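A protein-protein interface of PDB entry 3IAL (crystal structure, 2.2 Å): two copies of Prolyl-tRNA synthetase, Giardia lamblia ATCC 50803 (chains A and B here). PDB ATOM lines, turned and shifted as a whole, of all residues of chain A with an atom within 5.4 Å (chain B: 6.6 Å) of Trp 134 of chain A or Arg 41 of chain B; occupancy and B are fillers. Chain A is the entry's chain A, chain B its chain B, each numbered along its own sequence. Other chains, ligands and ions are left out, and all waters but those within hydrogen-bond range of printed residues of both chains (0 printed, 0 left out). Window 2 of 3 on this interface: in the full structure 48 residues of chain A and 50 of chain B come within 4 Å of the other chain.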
ATOM      1  N   ILE A  77     -22.256 -19.610  31.670  1.00  0.00           N
ATOM      2  CA  ILE A  77     -21.115 -19.486  30.782  1.00  0.00           C
ATOM      3  C   ILE A  77     -19.822 -19.748  31.562  1.00  0.00           C
ATOM      4  O   ILE A  77     -19.858 -19.980  32.764  1.00  0.00           O
ATOM      5  CB  ILE A  77     -21.025 -18.070  30.183  1.00  0.00           C
ATOM      6  CG1 ILE A  77     -20.783 -17.023  31.275  1.00  0.00           C
ATOM      7  CG2 ILE A  77     -22.278 -17.731  29.422  1.00  0.00           C
ATOM      8  CD1 ILE A  77     -20.459 -15.662  30.713  1.00  0.00           C
ATOM      9  N   PHE A  79     -15.854 -17.908  31.493  1.00  0.00           N
ATOM     10  CA  PHE A  79     -14.792 -17.043  31.018  1.00  0.00           C
ATOM     11  C   PHE A  79     -13.444 -17.576  31.477  1.00  0.00           C
ATOM     12  O   PHE A  79     -13.379 -18.362  32.409  1.00  0.00           O
ATOM     13  CB  PHE A  79     -14.960 -15.637  31.595  1.00  0.00           C
ATOM     14  CG  PHE A  79     -15.714 -14.706  30.709  1.00  0.00           C
ATOM     15  CD1 PHE A  79     -17.064 -14.877  30.489  1.00  0.00           C
ATOM     16  CD2 PHE A  79     -15.067 -13.644  30.103  1.00  0.00           C
ATOM     17  CE1 PHE A  79     -17.759 -14.004  29.664  1.00  0.00           C
ATOM     18  CE2 PHE A  79     -15.751 -12.778  29.288  1.00  0.00           C
ATOM     19  CZ  PHE A  79     -17.099 -12.961  29.061  1.00  0.00           C
ATOM     20  N   ILE A 127     -15.729  -9.545  31.476  1.00  0.00           N
ATOM     21  CA  ILE A 127     -17.059  -9.794  30.956  1.00  0.00           C
ATOM     22  C   ILE A 127     -17.595  -8.611  30.146  1.00  0.00           C
ATOM     23  O   ILE A 127     -18.162  -8.813  29.072  1.00  0.00           O
ATOM     24  CB  ILE A 127     -18.019 -10.198  32.097  1.00  0.00           C
ATOM     25  CG1 ILE A 127     -17.606 -11.577  32.634  1.00  0.00           C
ATOM     26  CG2 ILE A 127     -19.478 -10.191  31.618  1.00  0.00           C
ATOM     27  CD1 ILE A 127     -18.518 -12.140  33.684  1.00  0.00           C
ATOM     28  N   MET A 130     -16.361  -8.187  26.659  1.00  0.00           N
ATOM     29  CA  MET A 130     -17.037  -9.095  25.731  1.00  0.00           C
ATOM     30  C   MET A 130     -18.484  -8.668  25.439  1.00  0.00           C
ATOM     31  O   MET A 130     -18.954  -8.815  24.313  1.00  0.00           O
ATOM     32  CB  MET A 130     -16.982 -10.526  26.264  1.00  0.00           C
ATOM     33  CG  MET A 130     -15.571 -11.083  26.402  1.00  0.00           C
ATOM     34  SD  MET A 130     -14.549 -11.006  24.901  1.00  0.00           S
ATOM     35  CE  MET A 130     -15.474 -12.062  23.789  1.00  0.00           C
ATOM     36  N   PHE A 131     -19.176  -8.124  26.439  1.00  0.00           N
ATOM     37  CA  PHE A 131     -20.485  -7.498  26.215  1.00  0.00           C
ATOM     38  C   PHE A 131     -20.398  -6.438  25.112  1.00  0.00           C
ATOM     39  O   PHE A 131     -21.308  -6.307  24.293  1.00  0.00           O
ATOM     40  CB  PHE A 131     -21.001  -6.844  27.507  1.00  0.00           C
ATOM     41  CG  PHE A 131     -21.591  -7.806  28.512  1.00  0.00           C
ATOM     42  CD1 PHE A 131     -21.444  -9.185  28.391  1.00  0.00           C
ATOM     43  CD2 PHE A 131     -22.276  -7.310  29.616  1.00  0.00           C
ATOM     44  CE1 PHE A 131     -21.995 -10.040  29.325  1.00  0.00           C
ATOM     45  CE2 PHE A 131     -22.824  -8.162  30.554  1.00  0.00           C
ATOM     46  CZ  PHE A 131     -22.685  -9.524  30.415  1.00  0.00           C
ATOM     47  N   SER A 132     -19.305  -5.675  25.117  1.00  0.00           N
ATOM     48  CA  SER A 132     -19.012  -4.683  24.077  1.00  0.00           C
ATOM     49  C   SER A 132     -19.073  -5.278  22.664  1.00  0.00           C
ATOM     50  O   SER A 132     -19.573  -4.644  21.738  1.00  0.00           O
ATOM     51  CB  SER A 132     -17.617  -4.099  24.306  1.00  0.00           C
ATOM     52  OG  SER A 132     -17.364  -3.026  23.436  1.00  0.00           O
ATOM     53  N   LYS A 133     -18.543  -6.491  22.516  1.00  0.00           N
ATOM     54  CA  LYS A 133     -18.543  -7.200  21.240  1.00  0.00           C
ATOM     55  C   LYS A 133     -19.903  -7.842  20.946  1.00  0.00           C
ATOM     56  O   LYS A 133     -20.341  -7.851  19.809  1.00  0.00           O
ATOM     57  CB  LYS A 133     -17.446  -8.268  21.230  1.00  0.00           C
ATOM     58  CG  LYS A 133     -16.023  -7.707  21.258  1.00  0.00           C
ATOM     59  CD  LYS A 133     -15.023  -8.759  21.710  1.00  0.00           C
ATOM     60  CE  LYS A 133     -13.585  -8.396  21.377  1.00  0.00           C
ATOM     61  NZ  LYS A 133     -13.226  -6.984  21.664  1.00  0.00           N
ATOM     62  N   TRP A 134     -20.576  -8.362  21.972  1.00  0.00           N
ATOM     63  CA  TRP A 134     -21.825  -9.099  21.765  1.00  0.00           C
ATOM     64  C   TRP A 134     -23.062  -8.212  21.577  1.00  0.00           C
ATOM     65  O   TRP A 134     -24.056  -8.664  21.000  1.00  0.00           O
ATOM     66  CB  TRP A 134     -22.066 -10.084  22.912  1.00  0.00           C
ATOM     67  CG  TRP A 134     -20.978 -11.114  23.074  1.00  0.00           C
ATOM     68  CD1 TRP A 134     -20.144 -11.596  22.096  1.00  0.00           C
ATOM     69  CD2 TRP A 134     -20.639 -11.824  24.275  1.00  0.00           C
ATOM     70  NE1 TRP A 134     -19.296 -12.545  22.625  1.00  0.00           N
ATOM     71  CE2 TRP A 134     -19.580 -12.706  23.957  1.00  0.00           C
ATOM     72  CE3 TRP A 134     -21.125 -11.797  25.591  1.00  0.00           C
ATOM     73  CZ2 TRP A 134     -18.997 -13.547  24.904  1.00  0.00           C
ATOM     74  CZ3 TRP A 134     -20.543 -12.641  26.536  1.00  0.00           C
ATOM     75  CH2 TRP A 134     -19.487 -13.503  26.184  1.00  0.00           C
ATOM     76  N   VAL A 135     -23.010  -6.970  22.059  1.00  0.00           N
ATOM     77  CA  VAL A 135     -24.182  -6.077  22.029  1.00  0.00           C
ATOM     78  C   VAL A 135     -24.095  -5.079  20.876  1.00  0.00           C
ATOM     79  O   VAL A 135     -23.157  -4.282  20.797  1.00  0.00           O
ATOM     80  CB  VAL A 135     -24.351  -5.315  23.369  1.00  0.00           C
ATOM     81  CG1 VAL A 135     -25.592  -4.426  23.339  1.00  0.00           C
ATOM     82  CG2 VAL A 135     -24.437  -6.294  24.524  1.00  0.00           C
ATOM     83  N   ARG A 136     -25.072  -5.148  19.972  1.00  0.00           N
ATOM     84  CA  ARG A 136     -25.143  -4.245  18.818  1.00  0.00           C
ATOM     85  C   ARG A 136     -26.463  -3.494  18.772  1.00  0.00           C
ATOM     86  O   ARG A 136     -26.481  -2.305  18.460  1.00  0.00           O
ATOM     87  CB  ARG A 136     -24.967  -5.020  17.504  1.00  0.00           C
ATOM     88  CG  ARG A 136     -23.536  -5.503  17.224  1.00  0.00           C
ATOM     89  CD  ARG A 136     -22.603  -4.353  16.838  1.00  0.00           C
ATOM     90  NE  ARG A 136     -21.913  -3.776  17.993  1.00  0.00           N
ATOM     91  CZ  ARG A 136     -20.712  -4.151  18.442  1.00  0.00           C
ATOM     92  NH1 ARG A 136     -20.009  -5.111  17.843  1.00  0.00           N
ATOM     93  NH2 ARG A 136     -20.198  -3.545  19.504  1.00  0.00           N
ATOM     94  N   ASP A 140     -30.467  -7.606  21.047  1.00  0.00           N
ATOM     95  CA  ASP A 140     -29.481  -8.362  21.825  1.00  0.00           C
ATOM     96  C   ASP A 140     -29.721  -8.259  23.330  1.00  0.00           C
ATOM     97  O   ASP A 140     -29.022  -8.900  24.109  1.00  0.00           O
ATOM     98  CB  ASP A 140     -28.062  -7.871  21.522  1.00  0.00           C
ATOM     99  CG  ASP A 140     -27.706  -7.980  20.056  1.00  0.00           C
ATOM    100  OD1 ASP A 140     -28.078  -8.991  19.428  1.00  0.00           O
ATOM    101  OD2 ASP A 140     -27.044  -7.056  19.539  1.00  0.00           O
ATOM    102  N   LEU A 143     -29.207  -9.371  27.980  1.00  0.00           N
ATOM    103  CA  LEU A 143     -28.171 -10.394  27.936  1.00  0.00           C
ATOM    104  C   LEU A 143     -27.827 -10.726  29.378  1.00  0.00           C
ATOM    105  O   LEU A 143     -27.369  -9.858  30.128  1.00  0.00           O
ATOM    106  CB  LEU A 143     -26.951  -9.865  27.187  1.00  0.00           C
ATOM    107  CG  LEU A 143     -25.776 -10.799  26.918  1.00  0.00           C
ATOM    108  CD1 LEU A 143     -26.225 -12.146  26.391  1.00  0.00           C
ATOM    109  CD2 LEU A 143     -24.833 -10.122  25.921  1.00  0.00           C
ATOM    110  N   VAL B  38     -18.245 -20.628  21.265  1.00  0.00           N
ATOM    111  CA  VAL B  38     -17.108 -20.013  21.921  1.00  0.00           C
ATOM    112  C   VAL B  38     -16.855 -18.639  21.313  1.00  0.00           C
ATOM    113  O   VAL B  38     -17.386 -18.302  20.251  1.00  0.00           O
ATOM    114  CB  VAL B  38     -15.828 -20.852  21.745  1.00  0.00           C
ATOM    115  CG1 VAL B  38     -15.998 -22.235  22.366  1.00  0.00           C
ATOM    116  CG2 VAL B  38     -15.464 -20.959  20.275  1.00  0.00           C
ATOM    117  N   ASP B  39     -16.055 -17.842  22.005  1.00  0.00           N
ATOM    118  CA  ASP B  39     -15.563 -16.606  21.440  1.00  0.00           C
ATOM    119  C   ASP B  39     -14.045 -16.521  21.615  1.00  0.00           C
ATOM    120  O   ASP B  39     -13.548 -16.413  22.737  1.00  0.00           O
ATOM    121  CB  ASP B  39     -16.267 -15.405  22.062  1.00  0.00           C
ATOM    122  CG  ASP B  39     -16.184 -14.184  21.181  1.00  0.00           C
ATOM    123  OD1 ASP B  39     -15.118 -14.004  20.553  1.00  0.00           O
ATOM    124  OD2 ASP B  39     -17.172 -13.424  21.103  1.00  0.00           O
ATOM    125  N   ARG B  40     -13.338 -16.558  20.483  1.00  0.00           N
ATOM    126  CA  ARG B  40     -11.870 -16.542  20.432  1.00  0.00           C
ATOM    127  C   ARG B  40     -11.289 -15.137  20.555  1.00  0.00           C
ATOM    128  O   ARG B  40     -10.076 -14.977  20.662  1.00  0.00           O
ATOM    129  CB  ARG B  40     -11.364 -17.131  19.103  1.00  0.00           C
ATOM    130  CG  ARG B  40     -11.856 -18.527  18.779  1.00  0.00           C
ATOM    131  CD  ARG B  40     -11.399 -18.969  17.392  1.00  0.00           C
ATOM    132  NE  ARG B  40      -9.996 -19.388  17.359  1.00  0.00           N
ATOM    133  CZ  ARG B  40      -9.384 -19.905  16.292  1.00  0.00           C
ATOM    134  NH1 ARG B  40     -10.037 -20.066  15.145  1.00  0.00           N
ATOM    135  NH2 ARG B  40      -8.109 -20.265  16.369  1.00  0.00           N
ATOM    136  N   ARG B  41     -12.151 -14.117  20.524  1.00  0.00           N
ATOM    137  CA  ARG B  41     -11.708 -12.717  20.531  1.00  0.00           C
ATOM    138  C   ARG B  41     -11.292 -12.183  21.913  1.00  0.00           C
ATOM    139  O   ARG B  41     -11.002 -10.996  22.060  1.00  0.00           O
ATOM    140  CB  ARG B  41     -12.801 -11.817  19.937  1.00  0.00           C
ATOM    141  CG  ARG B  41     -13.131 -12.118  18.479  1.00  0.00           C
ATOM    142  CD  ARG B  41     -14.324 -11.303  17.995  1.00  0.00           C
ATOM    143  NE  ARG B  41     -15.561 -11.695  18.670  1.00  0.00           N
ATOM    144  CZ  ARG B  41     -16.749 -11.131  18.462  1.00  0.00           C
ATOM    145  NH1 ARG B  41     -16.883 -10.136  17.589  1.00  0.00           N
ATOM    146  NH2 ARG B  41     -17.813 -11.566  19.129  1.00  0.00           N
ATOM    147  N   TYR B  42     -11.283 -13.040  22.927  1.00  0.00           N
ATOM    148  CA  TYR B  42     -10.701 -12.686  24.213  1.00  0.00           C
ATOM    149  C   TYR B  42      -9.200 -12.486  23.995  1.00  0.00           C
ATOM    150  O   TYR B  42      -8.543 -13.376  23.457  1.00  0.00           O
ATOM    151  CB  TYR B  42     -10.949 -13.804  25.216  1.00  0.00           C
ATOM    152  CG  TYR B  42     -10.708 -13.414  26.648  1.00  0.00           C
ATOM    153  CD1 TYR B  42     -11.649 -12.659  27.348  1.00  0.00           C
ATOM    154  CD2 TYR B  42      -9.551 -13.803  27.307  1.00  0.00           C
ATOM    155  CE1 TYR B  42     -11.438 -12.299  28.666  1.00  0.00           C
ATOM    156  CE2 TYR B  42      -9.333 -13.446  28.630  1.00  0.00           C
ATOM    157  CZ  TYR B  42     -10.280 -12.696  29.300  1.00  0.00           C
ATOM    158  OH  TYR B  42     -10.070 -12.339  30.601  1.00  0.00           O
ATOM    159  N   PRO B  43      -8.652 -11.326  24.406  1.00  0.00           N
ATOM    160  CA  PRO B  43      -7.267 -10.971  24.087  1.00  0.00           C
ATOM    161  C   PRO B  43      -6.172 -11.695  24.897  1.00  0.00           C
ATOM    162  O   PRO B  43      -5.151 -11.103  25.210  1.00  0.00           O
ATOM    163  CB  PRO B  43      -7.234  -9.464  24.368  1.00  0.00           C
ATOM    164  CG  PRO B  43      -8.197  -9.298  25.468  1.00  0.00           C
ATOM    165  CD  PRO B  43      -9.319 -10.251  25.163  1.00  0.00           C
ATOM    166  N   VAL B  44      -6.379 -12.963  25.223  1.00  0.00           N
ATOM    167  CA  VAL B  44      -5.295 -13.792  25.725  1.00  0.00           C
ATOM    168  C   VAL B  44      -5.265 -15.032  24.844  1.00  0.00           C
ATOM    169  O   VAL B  44      -6.230 -15.794  24.819  1.00  0.00           O
ATOM    170  CB  VAL B  44      -5.481 -14.147  27.216  1.00  0.00           C
ATOM    171  CG1 VAL B  44      -4.364 -15.070  27.700  1.00  0.00           C
ATOM    172  CG2 VAL B  44      -5.510 -12.871  28.054  1.00  0.00           C
ATOM    173  N   CYS B  47      -7.042 -18.610  25.217  1.00  0.00           N
ATOM    174  CA  CYS B  47      -8.022 -18.548  26.299  1.00  0.00           C
ATOM    175  C   CYS B  47      -9.336 -18.073  25.703  1.00  0.00           C
ATOM    176  O   CYS B  47      -9.505 -16.880  25.426  1.00  0.00           O
ATOM    177  CB  CYS B  47      -7.567 -17.590  27.401  1.00  0.00           C
ATOM    178  SG  CYS B  47      -6.054 -18.084  28.206  1.00  0.00           S
ATOM    179  N   VAL B  48     -10.263 -19.005  25.500  1.00  0.00           N
ATOM    180  CA  VAL B  48     -11.482 -18.696  24.777  1.00  0.00           C
ATOM    181  C   VAL B  48     -12.662 -18.648  25.720  1.00  0.00           C
ATOM    182  O   VAL B  48     -12.744 -19.439  26.650  1.00  0.00           O
ATOM    183  CB  VAL B  48     -11.753 -19.721  23.644  1.00  0.00           C
ATOM    184  CG1 VAL B  48     -10.535 -19.833  22.736  1.00  0.00           C
ATOM    185  CG2 VAL B  48     -12.111 -21.067  24.219  1.00  0.00           C
ATOM    186  N   VAL B  49     -13.574 -17.711  25.470  1.00  0.00           N
ATOM    187  CA  VAL B  49     -14.814 -17.630  26.216  1.00  0.00           C
ATOM    188  C   VAL B  49     -15.730 -18.772  25.786  1.00  0.00           C
ATOM    189  O   VAL B  49     -15.927 -18.992  24.595  1.00  0.00           O
ATOM    190  CB  VAL B  49     -15.543 -16.279  25.976  1.00  0.00           C
ATOM    191  CG1 VAL B  49     -16.892 -16.231  26.723  1.00  0.00           C
ATOM    192  CG2 VAL B  49     -14.647 -15.108  26.393  1.00  0.00           C
ATOM    193  N   PHE B  50     -16.258 -19.510  26.759  1.00  0.00           N
ATOM    194  CA  PHE B  50     -17.361 -20.432  26.518  1.00  0.00           C
ATOM    195  C   PHE B  50     -18.664 -19.637  26.580  1.00  0.00           C
ATOM    196  O   PHE B  50     -19.081 -19.216  27.662  1.00  0.00           O
ATOM    197  CB  PHE B  50     -17.394 -21.533  27.581  1.00  0.00           C
ATOM    198  CG  PHE B  50     -16.881 -22.867  27.120  1.00  0.00           C
ATOM    199  CD1 PHE B  50     -17.522 -23.561  26.099  1.00  0.00           C
ATOM    200  CD2 PHE B  50     -15.798 -23.459  27.752  1.00  0.00           C
ATOM    201  CE1 PHE B  50     -17.065 -24.818  25.689  1.00  0.00           C
ATOM    202  CE2 PHE B  50     -15.335 -24.694  27.355  1.00  0.00           C
ATOM    203  CZ  PHE B  50     -15.974 -25.384  26.318  1.00  0.00           C
ATOM    204  N   ARG B  51     -19.314 -19.431  25.432  1.00  0.00           N
ATOM    205  CA  ARG B  51     -20.624 -18.767  25.408  1.00  0.00           C
ATOM    206  C   ARG B  51     -21.727 -19.758  25.817  1.00  0.00           C
ATOM    207  O   ARG B  51     -21.497 -20.966  25.802  1.00  0.00           O
ATOM    208  CB  ARG B  51     -20.881 -18.177  24.023  1.00  0.00           C
ATOM    209  CG  ARG B  51     -19.787 -17.223  23.574  1.00  0.00           C
ATOM    210  CD  ARG B  51     -20.147 -16.544  22.283  1.00  0.00           C
ATOM    211  NE  ARG B  51     -21.254 -15.608  22.449  1.00  0.00           N
ATOM    212  CZ  ARG B  51     -21.674 -14.768  21.506  1.00  0.00           C
ATOM    213  NH1 ARG B  51     -21.085 -14.749  20.311  1.00  0.00           N
ATOM    214  NH2 ARG B  51     -22.689 -13.950  21.758  1.00  0.00           N
ATOM    215  N   PRO B  52     -22.925 -19.255  26.183  1.00  0.00           N
ATOM    216  CA  PRO B  52     -23.979 -20.095  26.789  1.00  0.00           C
ATOM    217  C   PRO B  52     -24.314 -21.406  26.085  1.00  0.00           C
ATOM    218  O   PRO B  52     -24.372 -22.463  26.732  1.00  0.00           O
ATOM    219  CB  PRO B  52     -25.196 -19.175  26.767  1.00  0.00           C
ATOM    220  CG  PRO B  52     -24.629 -17.833  26.958  1.00  0.00           C
ATOM    221  CD  PRO B  52     -23.332 -17.837  26.181  1.00  0.00           C
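The indole nitrogen of Trp 134 of chain A is in hydrogen-bond range of the side-chain carboxylate of Asp 39 of chain B, 2.8 Å away.
O of Lys 133 of chain A sits at hydrogen-bond distance from NH1 of Arg 136 of chain A, 3.4 Å away. OD2 of Asp 39 of chain B lies within salt-bridge range of NH2 of Arg 41 of chain B (2.8 Å). N of Asp 39 of chain B sits at hydrogen-bond distance from O of Val 49 of chain B, 2.8 Å away.
Among the printed residues, pairs that only touch across the chains: Ile 77 of chain A with Phe 50 of chain B (3.4 Å), Ile 77 of chain A with Pro 52 of chain B (3.4 Å), Met 130 of chain A with Asp 39 of chain B (3.4 Å), Trp 134 of chain A with Arg 51 of chain B (3.4 Å), Lys 133 of chain A with Arg 41 of chain B (3.7 Å), Trp 134 of chain A with Arg 41 of chain B (3.8 Å), Phe 79 of chain A with Val 49 of chain B (3.8 Å) and Trp 134 of chain A with Val 49 of chain B (3.8 Å).
Of the printed residues of chain B, Ile 77 of chain A touches Phe 50 and Pro 52. Of the printed residues of chain B, Met 130 of chain A touches Asp 39. Of chain B, only Asp 39 (2.8 Å), Arg 41 (3.8 Å), Val 49 (3.8 Å) and Arg 51 (3.4 Å) come within 4 Å of Trp 134 of chain A. Val 38 of chain B touches none of the printed residues of chain A. Of chain A, only Lys 133 (3.7 Å) and Trp 134 (3.8 Å) come within 4 Å of Arg 41 of chain B. Val 48 of chain B touches none of the printed residues of chain A. Printed residues of chain A within 4 Å of Phe 50 of chain B: Ile 77. The nearest printed residue of chain A that does not touch Phe 50 of chain B is Phe 79 of chain A (5.0 Å).
Printed residues of chain B that touch a printed residue of chain A: Asp 39, Arg 41, Val 49, Phe 50, Arg 51 and Pro 52. Hydrophobic or aromatic side chains of chain B that line the printed part of chain A: Val 49 and Pro 52. Hydrophobic or aromatic side chains of chain A that line the printed part of chain B: Ile 77, Phe 79, Met 130 and Trp 134.
No position is printed for both chains. Of the 9 pairs that touch across the chains among the printed residues, none has its exchanged pair printed and touching as well.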
